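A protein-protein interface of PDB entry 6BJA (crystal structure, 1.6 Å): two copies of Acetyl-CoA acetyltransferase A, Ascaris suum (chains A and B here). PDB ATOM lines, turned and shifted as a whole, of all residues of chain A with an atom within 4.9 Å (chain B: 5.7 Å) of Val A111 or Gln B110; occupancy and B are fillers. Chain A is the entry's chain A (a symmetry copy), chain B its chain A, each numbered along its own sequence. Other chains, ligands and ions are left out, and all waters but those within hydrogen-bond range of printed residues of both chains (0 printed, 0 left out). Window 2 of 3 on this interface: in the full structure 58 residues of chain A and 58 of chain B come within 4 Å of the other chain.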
ATOM      1  N   LYS A   9      21.182 -11.995  -8.529  1.00  0.00           N
ATOM      2  CA  LYS A   9      20.293 -11.228  -9.400  1.00  0.00           C
ATOM      3  C   LYS A   9      19.542 -12.151 -10.367  1.00  0.00           C
ATOM      4  O   LYS A   9      19.056 -11.735 -11.423  1.00  0.00           O
ATOM      5  CB  LYS A   9      21.088 -10.173 -10.147  1.00  0.00           C
ATOM      6  CG  LYS A   9      21.879  -9.295  -9.202  1.00  0.00           C
ATOM      7  CD  LYS A   9      22.326  -8.000  -9.860  1.00  0.00           C
ATOM      8  CE  LYS A   9      23.275  -8.250 -11.016  1.00  0.00           C
ATOM      9  NZ  LYS A   9      23.608  -6.978 -11.700  1.00  0.00           N
ATOM     10  N   GLN A 107      13.881  -7.487 -15.676  1.00  0.00           N
ATOM     11  CA  GLN A 107      15.027  -6.656 -16.028  1.00  0.00           C
ATOM     12  C   GLN A 107      15.474  -5.777 -14.857  1.00  0.00           C
ATOM     13  O   GLN A 107      16.669  -5.643 -14.597  1.00  0.00           O
ATOM     14  CB  GLN A 107      14.703  -5.781 -17.240  1.00  0.00           C
ATOM     15  CG  GLN A 107      15.941  -5.193 -17.893  1.00  0.00           C
ATOM     16  CD  GLN A 107      15.611  -4.390 -19.150  1.00  0.00           C
ATOM     17  OE1 GLN A 107      15.266  -3.210 -19.068  1.00  0.00           O
ATOM     18  NE2 GLN A 107      15.700  -5.038 -20.316  1.00  0.00           N
ATOM     19  N   ALA A 108      14.523  -5.159 -14.159  1.00  0.00           N
ATOM     20  CA  ALA A 108      14.848  -4.329 -13.005  1.00  0.00           C
ATOM     21  C   ALA A 108      15.669  -5.096 -11.978  1.00  0.00           C
ATOM     22  O   ALA A 108      16.562  -4.550 -11.330  1.00  0.00           O
ATOM     23  CB  ALA A 108      13.587  -3.791 -12.378  1.00  0.00           C
ATOM     24  N   ILE A 109      15.330  -6.365 -11.795  1.00  0.00           N
ATOM     25  CA  ILE A 109      16.060  -7.225 -10.878  1.00  0.00           C
ATOM     26  C   ILE A 109      17.409  -7.640 -11.467  1.00  0.00           C
ATOM     27  O   ILE A 109      18.437  -7.600 -10.780  1.00  0.00           O
ATOM     28  CB  ILE A 109      15.198  -8.462 -10.522  1.00  0.00           C
ATOM     29  CG1 ILE A 109      14.042  -8.019  -9.629  1.00  0.00           C
ATOM     30  CG2 ILE A 109      16.005  -9.537  -9.817  1.00  0.00           C
ATOM     31  CD1 ILE A 109      12.954  -9.081  -9.419  1.00  0.00           C
ATOM     32  N   GLN A 110      17.412  -8.023 -12.743  1.00  0.00           N
ATOM     33  CA  GLN A 110      18.629  -8.468 -13.408  1.00  0.00           C
ATOM     34  C   GLN A 110      19.730  -7.424 -13.314  1.00  0.00           C
ATOM     35  O   GLN A 110      20.889  -7.760 -13.114  1.00  0.00           O
ATOM     36  CB  GLN A 110      18.358  -8.780 -14.878  1.00  0.00           C
ATOM     37  CG  GLN A 110      17.558 -10.034 -15.081  1.00  0.00           C
ATOM     38  CD  GLN A 110      17.129 -10.242 -16.523  1.00  0.00           C
ATOM     39  OE1 GLN A 110      17.048  -9.291 -17.317  1.00  0.00           O
ATOM     40  NE2 GLN A 110      16.874 -11.497 -16.875  1.00  0.00           N
ATOM     41  N   VAL A 111      19.344  -6.160 -13.435  1.00  0.00           N
ATOM     42  CA  VAL A 111      20.306  -5.072 -13.532  1.00  0.00           C
ATOM     43  C   VAL A 111      20.719  -4.590 -12.137  1.00  0.00           C
ATOM     44  O   VAL A 111      21.606  -3.735 -12.008  1.00  0.00           O
ATOM     45  CB  VAL A 111      19.729  -3.911 -14.375  1.00  0.00           C
ATOM     46  CG1 VAL A 111      18.776  -3.041 -13.570  1.00  0.00           C
ATOM     47  CG2 VAL A 111      20.844  -3.067 -14.981  1.00  0.00           C
ATOM     48  N   GLY A 112      20.071  -5.127 -11.103  1.00  0.00           N
ATOM     49  CA  GLY A 112      20.419  -4.840  -9.715  1.00  0.00           C
ATOM     50  C   GLY A 112      19.749  -3.604  -9.131  1.00  0.00           C
ATOM     51  O   GLY A 112      20.042  -3.203  -8.004  1.00  0.00           O
ATOM     52  N   TYR A 113      18.852  -2.989  -9.894  1.00  0.00           N
ATOM     53  CA  TYR A 113      18.152  -1.790  -9.450  1.00  0.00           C
ATOM     54  C   TYR A 113      17.118  -2.114  -8.390  1.00  0.00           C
ATOM     55  O   TYR A 113      16.980  -1.389  -7.398  1.00  0.00           O
ATOM     56  CB  TYR A 113      17.477  -1.113 -10.625  1.00  0.00           C
ATOM     57  CG  TYR A 113      16.788   0.182 -10.315  1.00  0.00           C
ATOM     58  CD1 TYR A 113      17.436   1.190  -9.608  1.00  0.00           C
ATOM     59  CD2 TYR A 113      15.516   0.444 -10.794  1.00  0.00           C
ATOM     60  CE1 TYR A 113      16.820   2.384  -9.360  1.00  0.00           C
ATOM     61  CE2 TYR A 113      14.892   1.633 -10.554  1.00  0.00           C
ATOM     62  CZ  TYR A 113      15.552   2.608  -9.825  1.00  0.00           C
ATOM     63  OH  TYR A 113      14.936   3.801  -9.580  1.00  0.00           O
ATOM     64  N   LYS B   9      28.796  -0.922 -21.647  1.00  0.00           N
ATOM     65  CA  LYS B   9      27.371  -0.781 -21.353  1.00  0.00           C
ATOM     66  C   LYS B   9      27.085   0.548 -20.644  1.00  0.00           C
ATOM     67  O   LYS B   9      26.070   0.721 -19.961  1.00  0.00           O
ATOM     68  CB  LYS B   9      26.897  -1.962 -20.526  1.00  0.00           C
ATOM     69  CG  LYS B   9      27.227  -3.280 -21.190  1.00  0.00           C
ATOM     70  CD  LYS B   9      26.410  -4.429 -20.625  1.00  0.00           C
ATOM     71  CE  LYS B   9      26.709  -4.670 -19.159  1.00  0.00           C
ATOM     72  NZ  LYS B   9      25.822  -5.724 -18.612  1.00  0.00           N
ATOM     73  N   VAL B  11      25.936   4.404 -21.041  1.00  0.00           N
ATOM     74  CA  VAL B  11      24.808   4.925 -21.802  1.00  0.00           C
ATOM     75  C   VAL B  11      25.084   6.331 -22.314  1.00  0.00           C
ATOM     76  O   VAL B  11      25.295   7.256 -21.536  1.00  0.00           O
ATOM     77  CB  VAL B  11      23.540   4.948 -20.929  1.00  0.00           C
ATOM     78  CG1 VAL B  11      22.351   5.506 -21.683  1.00  0.00           C
ATOM     79  CG2 VAL B  11      23.220   3.546 -20.428  1.00  0.00           C
ATOM     80  N   ILE B 103      14.742   6.463 -18.918  1.00  0.00           N
ATOM     81  CA  ILE B 103      15.312   5.575 -17.910  1.00  0.00           C
ATOM     82  C   ILE B 103      15.206   4.101 -18.359  1.00  0.00           C
ATOM     83  O   ILE B 103      16.164   3.343 -18.220  1.00  0.00           O
ATOM     84  CB  ILE B 103      14.639   5.824 -16.544  1.00  0.00           C
ATOM     85  CG1 ILE B 103      15.101   7.181 -16.015  1.00  0.00           C
ATOM     86  CG2 ILE B 103      15.008   4.713 -15.561  1.00  0.00           C
ATOM     87  CD1 ILE B 103      14.262   7.706 -14.873  1.00  0.00           C
ATOM     88  N   GLY B 105      15.161   3.047 -21.415  1.00  0.00           N
ATOM     89  CA  GLY B 105      16.117   2.861 -22.486  1.00  0.00           C
ATOM     90  C   GLY B 105      17.506   2.686 -21.919  1.00  0.00           C
ATOM     91  O   GLY B 105      18.259   1.837 -22.368  1.00  0.00           O
ATOM     92  N   ALA B 106      17.852   3.505 -20.927  1.00  0.00           N
ATOM     93  CA  ALA B 106      19.155   3.400 -20.286  1.00  0.00           C
ATOM     94  C   ALA B 106      19.294   2.025 -19.633  1.00  0.00           C
ATOM     95  O   ALA B 106      20.329   1.389 -19.748  1.00  0.00           O
ATOM     96  CB  ALA B 106      19.358   4.514 -19.260  1.00  0.00           C
ATOM     97  N   GLN B 107      18.251   1.572 -18.947  1.00  0.00           N
ATOM     98  CA  GLN B 107      18.309   0.269 -18.295  1.00  0.00           C
ATOM     99  C   GLN B 107      18.509  -0.865 -19.304  1.00  0.00           C
ATOM    100  O   GLN B 107      19.300  -1.778 -19.069  1.00  0.00           O
ATOM    101  CB  GLN B 107      17.039   0.019 -17.481  1.00  0.00           C
ATOM    102  CG  GLN B 107      17.189  -1.114 -16.480  1.00  0.00           C
ATOM    103  CD  GLN B 107      15.943  -1.299 -15.616  1.00  0.00           C
ATOM    104  OE1 GLN B 107      14.994  -1.971 -16.022  1.00  0.00           O
ATOM    105  NE2 GLN B 107      15.940  -0.685 -14.429  1.00  0.00           N
ATOM    106  N   ALA B 108      17.784  -0.825 -20.420  1.00  0.00           N
ATOM    107  CA  ALA B 108      17.931  -1.841 -21.457  1.00  0.00           C
ATOM    108  C   ALA B 108      19.376  -1.962 -21.919  1.00  0.00           C
ATOM    109  O   ALA B 108      19.865  -3.050 -22.222  1.00  0.00           O
ATOM    110  CB  ALA B 108      17.028  -1.529 -22.623  1.00  0.00           C
ATOM    111  N   ILE B 109      20.051  -0.826 -22.017  1.00  0.00           N
ATOM    112  CA  ILE B 109      21.452  -0.802 -22.403  1.00  0.00           C
ATOM    113  C   ILE B 109      22.349  -1.267 -21.256  1.00  0.00           C
ATOM    114  O   ILE B 109      23.267  -2.070 -21.457  1.00  0.00           O
ATOM    115  CB  ILE B 109      21.841   0.622 -22.877  1.00  0.00           C
ATOM    116  CG1 ILE B 109      21.176   0.893 -24.224  1.00  0.00           C
ATOM    117  CG2 ILE B 109      23.345   0.790 -23.008  1.00  0.00           C
ATOM    118  CD1 ILE B 109      21.246   2.354 -24.689  1.00  0.00           C
ATOM    119  N   GLN B 110      22.074  -0.778 -20.047  1.00  0.00           N
ATOM    120  CA  GLN B 110      22.874  -1.124 -18.880  1.00  0.00           C
ATOM    121  C   GLN B 110      22.948  -2.629 -18.681  1.00  0.00           C
ATOM    122  O   GLN B 110      23.995  -3.158 -18.330  1.00  0.00           O
ATOM    123  CB  GLN B 110      22.298  -0.479 -17.620  1.00  0.00           C
ATOM    124  CG  GLN B 110      22.508   1.006 -17.564  1.00  0.00           C
ATOM    125  CD  GLN B 110      21.775   1.670 -16.413  1.00  0.00           C
ATOM    126  OE1 GLN B 110      20.784   1.140 -15.885  1.00  0.00           O
ATOM    127  NE2 GLN B 110      22.276   2.828 -15.999  1.00  0.00           N
ATOM    128  N   VAL B 111      21.834  -3.305 -18.933  1.00  0.00           N
ATOM    129  CA  VAL B 111      21.713  -4.722 -18.626  1.00  0.00           C
ATOM    130  C   VAL B 111      22.240  -5.574 -19.788  1.00  0.00           C
ATOM    131  O   VAL B 111      22.313  -6.805 -19.678  1.00  0.00           O
ATOM    132  CB  VAL B 111      20.246  -5.081 -18.293  1.00  0.00           C
ATOM    133  CG1 VAL B 111      19.400  -5.246 -19.547  1.00  0.00           C
ATOM    134  CG2 VAL B 111      20.172  -6.334 -17.428  1.00  0.00           C
ATOM    135  N   GLY B 112      22.593  -4.920 -20.896  1.00  0.00           N
ATOM    136  CA  GLY B 112      23.201  -5.582 -22.045  1.00  0.00           C
ATOM    137  C   GLY B 112      22.210  -6.167 -23.042  1.00  0.00           C
ATOM    138  O   GLY B 112      22.602  -6.837 -24.000  1.00  0.00           O
ATOM    139  N   TYR B 113      20.923  -5.925 -22.824  1.00  0.00           N
ATOM    140  CA  TYR B 113      19.880  -6.440 -23.702  1.00  0.00           C
ATOM    141  C   TYR B 113      19.856  -5.702 -25.026  1.00  0.00           C
ATOM    142  O   TYR B 113      19.706  -6.313 -26.090  1.00  0.00           O
ATOM    143  CB  TYR B 113      18.527  -6.321 -23.034  1.00  0.00           C
ATOM    144  CG  TYR B 113      17.373  -6.894 -23.803  1.00  0.00           C
ATOM    145  CD1 TYR B 113      17.430  -8.179 -24.334  1.00  0.00           C
ATOM    146  CD2 TYR B 113      16.188  -6.191 -23.936  1.00  0.00           C
ATOM    147  CE1 TYR B 113      16.364  -8.712 -25.000  1.00  0.00           C
ATOM    148  CE2 TYR B 113      15.117  -6.716 -24.599  1.00  0.00           C
ATOM    149  CZ  TYR B 113      15.212  -7.986 -25.138  1.00  0.00           C
ATOM    150  OH  TYR B 113      14.145  -8.520 -25.804  1.00  0.00           O
ATOM    151  N   ARG B 114      19.998  -4.382 -24.943  1.00  0.00           N
ATOM    152  CA  ARG B 114      20.008  -3.514 -26.131  1.00  0.00           C
ATOM    153  C   ARG B 114      21.295  -2.720 -26.263  1.00  0.00           C
ATOM    154  O   ARG B 114      21.996  -2.466 -25.276  1.00  0.00           O
ATOM    155  CB  ARG B 114      18.852  -2.513 -26.086  1.00  0.00           C
ATOM    156  CG  ARG B 114      17.491  -3.103 -25.995  1.00  0.00           C
ATOM    157  CD  ARG B 114      17.200  -4.068 -27.111  1.00  0.00           C
ATOM    158  NE  ARG B 114      15.794  -4.435 -27.141  1.00  0.00           N
ATOM    159  CZ  ARG B 114      15.269  -5.331 -27.961  1.00  0.00           C
ATOM    160  NH1 ARG B 114      16.043  -5.950 -28.852  1.00  0.00           N
ATOM    161  NH2 ARG B 114      13.977  -5.602 -27.924  1.00  0.00           N
ATOM    162  N   LEU B 283      24.736   9.411 -16.538  1.00  0.00           N
ATOM    163  CA  LEU B 283      25.563   8.907 -15.443  1.00  0.00           C
ATOM    164  C   LEU B 283      24.771   8.100 -14.432  1.00  0.00           C
ATOM    165  O   LEU B 283      25.271   7.107 -13.891  1.00  0.00           O
ATOM    166  CB  LEU B 283      26.243  10.054 -14.727  1.00  0.00           C
ATOM    167  CG  LEU B 283      27.251  10.847 -15.545  1.00  0.00           C
ATOM    168  CD1 LEU B 283      27.894  11.884 -14.654  1.00  0.00           C
ATOM    169  CD2 LEU B 283      28.290   9.933 -16.175  1.00  0.00           C
ATOM    170  N   TYR B 285      20.407   7.740 -12.530  1.00  0.00           N
ATOM    171  CA  TYR B 285      19.034   8.194 -12.400  1.00  0.00           C
ATOM    172  C   TYR B 285      18.500   7.775 -11.030  1.00  0.00           C
ATOM    173  O   TYR B 285      19.057   6.888 -10.380  1.00  0.00           O
ATOM    174  CB  TYR B 285      18.162   7.631 -13.524  1.00  0.00           C
ATOM    175  CG  TYR B 285      18.050   6.148 -13.509  1.00  0.00           C
ATOM    176  CD1 TYR B 285      17.107   5.557 -12.698  1.00  0.00           C
ATOM    177  CD2 TYR B 285      18.870   5.343 -14.280  1.00  0.00           C
ATOM    178  CE1 TYR B 285      16.966   4.242 -12.637  1.00  0.00           C
ATOM    179  CE2 TYR B 285      18.729   3.957 -14.222  1.00  0.00           C
ATOM    180  CZ  TYR B 285      17.762   3.436 -13.381  1.00  0.00           C
ATOM    181  OH  TYR B 285      17.527   2.086 -13.237  1.00  0.00           O
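OE1 of Gln B107 sits close to OE1 of Gln A107 (3.3 Å).
The side-chain amino group (NZ) of Lys B9 is in hydrogen-bond range of the backbone carbonyl oxygen (O) of Gln B110 (3.2 Å). NE2 of Gln B107 is in hydrogen-bond range of OH of Tyr B285, 3.4 Å away. The backbone NH of Tyr B113 lies within hydrogen-bond range of the backbone carbonyl oxygen of Ala B108 (3.1 Å). N of Arg B114 sits at hydrogen-bond distance from O of Ala B108 (3.0 Å). NZ of Lys A9 sits at hydrogen-bond distance from O of Gln A110. The backbone carbonyl oxygen of Ala A108 sits at hydrogen-bond distance from the backbone NH of Tyr A113, 3.1 Å away.
Among the printed residues, pairs that only touch across the chains: Tyr A113 with Tyr B285 (3.5 Å), Ala A108 with Gln B107 (3.7 Å), Gln A107 with Ala B108 (3.7 Å), Gln A107 with Val B111 (3.8 Å), Val A111 with Gln B107 (3.8 Å), Tyr A113 with Gln B107 (3.8 Å), Gln A107 with Tyr B113 (3.8 Å), Val A111 with Val B111 (3.9 Å), Gln A110 with Val B111 (3.97 Å) and Val A111 with Gln B110 (3.97 Å).
Gln B110 touches just one residue of chain A: Val A111 (3.97 Å). Of the printed residues of chain A, Val B111 touches Gln A107 (3.8 Å), Gln A110 (3.97 Å) and Val A111 (3.9 Å). Of the printed residues of chain A, Ala B108 touches Gln A107. Of the printed residues of chain A, Gln B107 touches Gln A107, Ala A108, Val A111 and Tyr A113. Printed residues of chain A within 4 Å of Tyr B113: Gln A107. Of the printed residues of chain B, Ala A108 touches Gln B107. Lys A9 touches none of the printed residues of chain B. The nearest printed residue of chain A that does not touch Gln B110 is Tyr A113 (6.6 Å). The nearest printed residue of chain A that does not touch Tyr B113 is Gln A110 (6.6 Å).
Of the 15 printed residues of chain B, 6 touch a printed residue of chain A. Hydrophobic or aromatic side chains of chain B within 4 Å of the printed part of chain A: Val B111, Tyr B113 and Tyr B285. Along chain B the printed residues that touch a printed residue of chain A span positions 107 to 285. Printed residues of chain A that touch a printed residue of chain B: Gln A107, Ala A108, Gln A110, Val A111 and Tyr A113. Hydrophobic or aromatic side chains of chain A that line the printed part of chain B: Val A111 and Tyr A113. Among the printed residues, 11 pairs touch across the chains.
Gln B107 touches its own counterpart, Gln A107. Gln A107 touches Ala B108, and with the chains exchanged Ala A108 touches Gln B107. Gln A107 touches Val B111, and with the chains exchanged Val A111 touches Gln B107. Gln A107 touches Tyr B113, and with the chains exchanged Tyr A113 touches Gln B107. 8 positions are printed for both chains.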
